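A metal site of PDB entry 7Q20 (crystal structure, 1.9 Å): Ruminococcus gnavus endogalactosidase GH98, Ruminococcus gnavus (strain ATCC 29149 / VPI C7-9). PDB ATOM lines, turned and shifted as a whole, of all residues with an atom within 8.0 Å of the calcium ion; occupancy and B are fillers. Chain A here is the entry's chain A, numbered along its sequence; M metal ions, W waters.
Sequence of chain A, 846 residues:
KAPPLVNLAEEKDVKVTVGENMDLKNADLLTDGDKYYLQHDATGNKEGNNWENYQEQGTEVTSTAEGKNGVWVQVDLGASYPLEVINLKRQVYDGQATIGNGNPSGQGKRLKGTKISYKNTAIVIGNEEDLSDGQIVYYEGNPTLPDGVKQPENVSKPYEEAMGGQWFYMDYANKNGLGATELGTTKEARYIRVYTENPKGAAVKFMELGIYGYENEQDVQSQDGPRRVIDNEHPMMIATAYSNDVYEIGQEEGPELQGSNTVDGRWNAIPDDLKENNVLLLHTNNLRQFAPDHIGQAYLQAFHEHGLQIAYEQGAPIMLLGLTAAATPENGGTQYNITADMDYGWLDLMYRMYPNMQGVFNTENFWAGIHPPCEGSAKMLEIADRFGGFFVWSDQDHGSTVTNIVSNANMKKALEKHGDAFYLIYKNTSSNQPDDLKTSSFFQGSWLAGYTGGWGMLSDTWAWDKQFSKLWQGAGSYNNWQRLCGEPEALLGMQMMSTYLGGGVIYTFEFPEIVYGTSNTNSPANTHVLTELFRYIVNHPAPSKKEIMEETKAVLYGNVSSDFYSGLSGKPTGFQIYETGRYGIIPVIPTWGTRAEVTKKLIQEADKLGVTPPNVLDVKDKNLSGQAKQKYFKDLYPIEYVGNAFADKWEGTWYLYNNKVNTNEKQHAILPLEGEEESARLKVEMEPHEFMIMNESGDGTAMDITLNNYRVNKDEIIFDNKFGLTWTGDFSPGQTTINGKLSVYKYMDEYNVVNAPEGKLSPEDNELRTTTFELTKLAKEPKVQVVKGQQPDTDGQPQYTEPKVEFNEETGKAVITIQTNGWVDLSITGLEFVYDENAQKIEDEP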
ATOM      1  N   LEU A 501      17.253  36.107 -11.635  1.00  0.00           N
ATOM      2  CA  LEU A 501      17.819  34.760 -11.453  1.00  0.00           C
ATOM      3  C   LEU A 501      19.293  34.676 -11.834  1.00  0.00           C
ATOM      4  O   LEU A 501      20.007  33.837 -11.335  1.00  0.00           O
ATOM      5  CB  LEU A 501      17.001  33.703 -12.193  1.00  0.00           C
ATOM      6  CG  LEU A 501      15.588  33.510 -11.636  1.00  0.00           C
ATOM      7  CD1 LEU A 501      14.750  32.710 -12.597  1.00  0.00           C
ATOM      8  CD2 LEU A 501      15.654  32.809 -10.272  1.00  0.00           C
ATOM      9  N   GLU A 551      27.008  27.959  -8.500  1.00  0.00           N
ATOM     10  CA  GLU A 551      26.123  27.258  -9.443  1.00  0.00           C
ATOM     11  C   GLU A 551      26.671  27.135 -10.875  1.00  0.00           C
ATOM     12  O   GLU A 551      26.202  26.304 -11.651  1.00  0.00           O
ATOM     13  CB  GLU A 551      24.746  27.939  -9.503  1.00  0.00           C
ATOM     14  CG  GLU A 551      23.994  27.889  -8.183  1.00  0.00           C
ATOM     15  CD  GLU A 551      22.633  27.214  -8.335  1.00  0.00           C
ATOM     16  OE1 GLU A 551      22.587  26.034  -8.758  1.00  0.00           O
ATOM     17  OE2 GLU A 551      21.618  27.859  -8.029  1.00  0.00           O
ATOM     18  N   GLY A 581      15.658  27.297 -17.285  1.00  0.00           N
ATOM     19  CA  GLY A 581      16.622  27.875 -16.356  1.00  0.00           C
ATOM     20  C   GLY A 581      17.719  26.897 -15.955  1.00  0.00           C
ATOM     21  O   GLY A 581      18.524  27.173 -15.095  1.00  0.00           O
ATOM     22  N   ARG A 582      17.773  25.756 -16.651  1.00  0.00           N
ATOM     23  CA  ARG A 582      18.612  24.586 -16.278  1.00  0.00           C
ATOM     24  C   ARG A 582      20.080  24.992 -16.248  1.00  0.00           C
ATOM     25  O   ARG A 582      20.804  24.482 -15.406  1.00  0.00           O
ATOM     26  CB  ARG A 582      18.385  23.457 -17.279  1.00  0.00           C
ATOM     27  CG  ARG A 582      19.237  22.225 -17.042  1.00  0.00           C
ATOM     28  CD  ARG A 582      18.888  21.150 -18.030  1.00  0.00           C
ATOM     29  NE  ARG A 582      19.736  19.984 -17.868  1.00  0.00           N
ATOM     30  CZ  ARG A 582      19.546  18.833 -18.500  1.00  0.00           C
ATOM     31  NH1 ARG A 582      18.558  18.716 -19.372  1.00  0.00           N
ATOM     32  NH2 ARG A 582      20.367  17.823 -18.281  1.00  0.00           N
ATOM     33  N   TYR A 583      20.504  25.841 -17.183  1.00  0.00           N
ATOM     34  CA  TYR A 583      21.924  26.199 -17.427  1.00  0.00           C
ATOM     35  C   TYR A 583      22.217  27.620 -16.901  1.00  0.00           C
ATOM     36  O   TYR A 583      23.380  28.040 -17.008  1.00  0.00           O
ATOM     37  CB  TYR A 583      22.239  26.081 -18.917  1.00  0.00           C
ATOM     38  CG  TYR A 583      21.730  24.810 -19.548  1.00  0.00           C
ATOM     39  CD1 TYR A 583      22.329  23.592 -19.269  1.00  0.00           C
ATOM     40  CD2 TYR A 583      20.651  24.810 -20.417  1.00  0.00           C
ATOM     41  CE1 TYR A 583      21.877  22.417 -19.849  1.00  0.00           C
ATOM     42  CE2 TYR A 583      20.195  23.647 -21.009  1.00  0.00           C
ATOM     43  CZ  TYR A 583      20.796  22.440 -20.710  1.00  0.00           C
ATOM     44  OH  TYR A 583      20.370  21.274 -21.288  1.00  0.00           O
ATOM     45  N   GLY A 584      21.199  28.324 -16.387  1.00  0.00           N
ATOM     46  CA  GLY A 584      21.349  29.719 -16.027  1.00  0.00           C
ATOM     47  C   GLY A 584      21.563  30.592 -17.270  1.00  0.00           C
ATOM     48  O   GLY A 584      21.163  30.230 -18.381  1.00  0.00           O
ATOM     49  N   TYR A 637      24.970  20.070 -15.824  1.00  0.00           N
ATOM     50  CA  TYR A 637      23.753  20.656 -15.214  1.00  0.00           C
ATOM     51  C   TYR A 637      22.611  19.643 -15.248  1.00  0.00           C
ATOM     52  O   TYR A 637      22.076  19.364 -16.320  1.00  0.00           O
ATOM     53  CB  TYR A 637      23.371  21.945 -15.937  1.00  0.00           C
ATOM     54  CG  TYR A 637      24.387  23.048 -15.822  1.00  0.00           C
ATOM     55  CD1 TYR A 637      24.461  23.831 -14.674  1.00  0.00           C
ATOM     56  CD2 TYR A 637      25.245  23.328 -16.862  1.00  0.00           C
ATOM     57  CE1 TYR A 637      25.360  24.887 -14.580  1.00  0.00           C
ATOM     58  CE2 TYR A 637      26.160  24.367 -16.775  1.00  0.00           C
ATOM     59  CZ  TYR A 637      26.208  25.161 -15.641  1.00  0.00           C
ATOM     60  OH  TYR A 637      27.129  26.163 -15.560  1.00  0.00           O
ATOM     61  N   PRO A 638      22.222  19.067 -14.095  1.00  0.00           N
ATOM     62  CA  PRO A 638      21.160  18.052 -14.080  1.00  0.00           C
ATOM     63  C   PRO A 638      19.793  18.670 -14.407  1.00  0.00           C
ATOM     64  O   PRO A 638      19.570  19.838 -14.075  1.00  0.00           O
ATOM     65  CB  PRO A 638      21.230  17.504 -12.644  1.00  0.00           C
ATOM     66  CG  PRO A 638      21.779  18.672 -11.841  1.00  0.00           C
ATOM     67  CD  PRO A 638      22.772  19.343 -12.760  1.00  0.00           C
ATOM     68  N   GLU A 640      16.001  19.575 -13.870  1.00  0.00           N
ATOM     69  CA  GLU A 640      15.267  19.910 -12.634  1.00  0.00           C
ATOM     70  C   GLU A 640      13.755  19.655 -12.739  1.00  0.00           C
ATOM     71  O   GLU A 640      13.080  19.456 -11.724  1.00  0.00           O
ATOM     72  CB  GLU A 640      15.458  21.375 -12.263  1.00  0.00           C
ATOM     73  CG  GLU A 640      16.886  21.812 -12.079  1.00  0.00           C
ATOM     74  CD  GLU A 640      16.996  23.218 -11.482  1.00  0.00           C
ATOM     75  OE1 GLU A 640      16.341  24.161 -11.991  1.00  0.00           O
ATOM     76  OE2 GLU A 640      17.739  23.370 -10.489  1.00  0.00           O
ATOM     77  N   TYR A 641      13.231  19.718 -13.973  1.00  0.00           N
ATOM     78  CA  TYR A 641      11.793  19.601 -14.321  1.00  0.00           C
ATOM     79  C   TYR A 641      11.648  19.131 -15.770  1.00  0.00           C
ATOM     80  O   TYR A 641      12.616  19.268 -16.556  1.00  0.00           O
ATOM     81  CB  TYR A 641      11.055  20.942 -14.170  1.00  0.00           C
ATOM     82  CG  TYR A 641      11.346  21.936 -15.270  1.00  0.00           C
ATOM     83  CD1 TYR A 641      12.549  22.646 -15.290  1.00  0.00           C
ATOM     84  CD2 TYR A 641      10.460  22.143 -16.303  1.00  0.00           C
ATOM     85  CE1 TYR A 641      12.825  23.560 -16.296  1.00  0.00           C
ATOM     86  CE2 TYR A 641      10.724  23.051 -17.320  1.00  0.00           C
ATOM     87  CZ  TYR A 641      11.923  23.764 -17.310  1.00  0.00           C
ATOM     88  OH  TYR A 641      12.207  24.653 -18.304  1.00  0.00           O
ATOM     89  N   ALA A 647      11.257  27.056 -16.289  1.00  0.00           N
ATOM     90  CA  ALA A 647      11.258  26.879 -14.845  1.00  0.00           C
ATOM     91  C   ALA A 647      12.692  26.857 -14.358  1.00  0.00           C
ATOM     92  O   ALA A 647      13.589  26.391 -15.062  1.00  0.00           O
ATOM     93  CB  ALA A 647      10.554  25.578 -14.437  1.00  0.00           C
ATOM     94  N   ASP A 648      12.888  27.346 -13.126  1.00  0.00           N
ATOM     95  CA  ASP A 648      14.165  27.331 -12.455  1.00  0.00           C
ATOM     96  C   ASP A 648      13.855  27.184 -10.978  1.00  0.00           C
ATOM     97  O   ASP A 648      13.077  27.967 -10.432  1.00  0.00           O
ATOM     98  CB  ASP A 648      14.937  28.636 -12.704  1.00  0.00           C
ATOM     99  CG  ASP A 648      16.373  28.592 -12.225  1.00  0.00           C
ATOM    100  OD1 ASP A 648      16.837  27.570 -11.712  1.00  0.00           O
ATOM    101  OD2 ASP A 648      17.069  29.615 -12.363  1.00  0.00           O
ATOM    102  N   LYS A 649      14.434  26.156 -10.351  1.00  0.00           N
ATOM    103  CA  LYS A 649      14.470  26.083  -8.900  1.00  0.00           C
ATOM    104  C   LYS A 649      15.785  26.706  -8.438  1.00  0.00           C
ATOM    105  O   LYS A 649      16.880  26.330  -8.924  1.00  0.00           O
ATOM    106  CB  LYS A 649      14.291  24.636  -8.373  1.00  0.00           C
ATOM    107  CG  LYS A 649      13.964  24.607  -6.875  1.00  0.00           C
ATOM    108  CD  LYS A 649      13.720  23.201  -6.307  1.00  0.00           C
ATOM    109  CE  LYS A 649      13.144  23.303  -4.897  1.00  0.00           C
ATOM    110  NZ  LYS A 649      12.804  21.995  -4.276  1.00  0.00           N
ATOM    111  N   TRP A 650      15.643  27.691  -7.540  1.00  0.00           N
ATOM    112  CA  TRP A 650      16.743  28.402  -6.916  1.00  0.00           C
ATOM    113  C   TRP A 650      16.421  28.655  -5.416  1.00  0.00           C
ATOM    114  O   TRP A 650      15.417  29.284  -5.087  1.00  0.00           O
ATOM    115  CB  TRP A 650      17.047  29.746  -7.634  1.00  0.00           C
ATOM    116  CG  TRP A 650      18.108  30.476  -6.905  1.00  0.00           C
ATOM    117  CD1 TRP A 650      19.393  30.067  -6.742  1.00  0.00           C
ATOM    118  CD2 TRP A 650      17.962  31.680  -6.153  1.00  0.00           C
ATOM    119  NE1 TRP A 650      20.066  30.960  -5.967  1.00  0.00           N
ATOM    120  CE2 TRP A 650      19.218  31.959  -5.574  1.00  0.00           C
ATOM    121  CE3 TRP A 650      16.908  32.561  -5.917  1.00  0.00           C
ATOM    122  CZ2 TRP A 650      19.442  33.064  -4.773  1.00  0.00           C
ATOM    123  CZ3 TRP A 650      17.144  33.694  -5.116  1.00  0.00           C
ATOM    124  CH2 TRP A 650      18.396  33.930  -4.565  1.00  0.00           C
ATOM    125  N   GLU A 651      17.276  28.131  -4.538  1.00  0.00           N
ATOM    126  CA  GLU A 651      17.155  28.227  -3.085  1.00  0.00           C
ATOM    127  C   GLU A 651      15.712  28.025  -2.581  1.00  0.00           C
ATOM    128  O   GLU A 651      15.137  28.916  -1.958  1.00  0.00           O
ATOM    129  CB  GLU A 651      17.732  29.565  -2.562  1.00  0.00           C
ATOM    130  CG  GLU A 651      19.262  29.711  -2.689  1.00  0.00           C
ATOM    131  CD  GLU A 651      20.075  28.701  -1.875  1.00  0.00           C
ATOM    132  OE1 GLU A 651      19.531  27.949  -1.031  1.00  0.00           O
ATOM    133  OE2 GLU A 651      21.315  28.669  -2.075  1.00  0.00           O
ATOM    134  N   THR A 653      12.813  27.779  -4.076  1.00  0.00           N
ATOM    135  CA  THR A 653      11.715  28.470  -4.740  1.00  0.00           C
ATOM    136  C   THR A 653      11.741  28.175  -6.231  1.00  0.00           C
ATOM    137  O   THR A 653      12.796  28.230  -6.871  1.00  0.00           O
ATOM    138  CB  THR A 653      11.789  29.985  -4.477  1.00  0.00           C
ATOM    139  OG1 THR A 653      11.829  30.185  -3.053  1.00  0.00           O
ATOM    140  CG2 THR A 653      10.571  30.720  -5.017  1.00  0.00           C
ATOM    141  N   TRP A 654      10.565  27.839  -6.777  1.00  0.00           N
ATOM    142  CA  TRP A 654      10.393  27.666  -8.197  1.00  0.00           C
ATOM    143  C   TRP A 654       9.936  28.957  -8.848  1.00  0.00           C
ATOM    144  O   TRP A 654       9.011  29.619  -8.351  1.00  0.00           O
ATOM    145  CB  TRP A 654       9.388  26.578  -8.493  1.00  0.00           C
ATOM    146  CG  TRP A 654       9.887  25.196  -8.266  1.00  0.00           C
ATOM    147  CD1 TRP A 654       9.654  24.428  -7.173  1.00  0.00           C
ATOM    148  CD2 TRP A 654      10.657  24.400  -9.175  1.00  0.00           C
ATOM    149  NE1 TRP A 654      10.239  23.189  -7.329  1.00  0.00           N
ATOM    150  CE2 TRP A 654      10.859  23.146  -8.556  1.00  0.00           C
ATOM    151  CE3 TRP A 654      11.206  24.630 -10.449  1.00  0.00           C
ATOM    152  CZ2 TRP A 654      11.567  22.108  -9.174  1.00  0.00           C
ATOM    153  CZ3 TRP A 654      11.913  23.614 -11.069  1.00  0.00           C
ATOM    154  CH2 TRP A 654      12.090  22.361 -10.422  1.00  0.00           C
ATOM    155  N   TYR A 655      10.608  29.320  -9.944  1.00  0.00           N
ATOM    156  CA  TYR A 655      10.298  30.477 -10.811  1.00  0.00           C
ATOM    157  C   TYR A 655       9.941  29.949 -12.200  1.00  0.00           C
ATOM    158  O   TYR A 655      10.772  29.229 -12.764  1.00  0.00           O
ATOM    159  CB  TYR A 655      11.494  31.431 -10.878  1.00  0.00           C
ATOM    160  CG  TYR A 655      11.943  31.906  -9.527  1.00  0.00           C
ATOM    161  CD1 TYR A 655      12.779  31.137  -8.736  1.00  0.00           C
ATOM    162  CD2 TYR A 655      11.491  33.113  -9.011  1.00  0.00           C
ATOM    163  CE1 TYR A 655      13.179  31.567  -7.488  1.00  0.00           C
ATOM    164  CE2 TYR A 655      11.871  33.552  -7.756  1.00  0.00           C
ATOM    165  CZ  TYR A 655      12.729  32.773  -6.992  1.00  0.00           C
ATOM    166  OH  TYR A 655      13.094  33.196  -5.758  1.00  0.00           O
HETATM  167 CA    CA M   1      18.307  25.947 -10.985  1.00  0.00          CA
HETATM  168  O   HOH W   1      19.474  25.031  -9.340  1.00  0.00           O
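Three residues have an atom within 4 Å of the calcium ion: Glu 640, Asp 648 and Lys 649.
The calcium ion is bound by water W1 (2.2 Å), the side-chain carboxylate (OD1) of Asp 648 (2.3 Å), the backbone carbonyl oxygen (O) of Lys 649 (2.5 Å), the side-chain carboxylate (OE2) of Glu 640 (2.7 Å) and the side-chain carboxylate (OE1) of Glu 640 (2.8 Å).
The calcium ion has five donor atoms within binding distance.
O of Tyr 655 sits at hydrogen-bond distance from N of Asp 648, at 2.9 Å.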
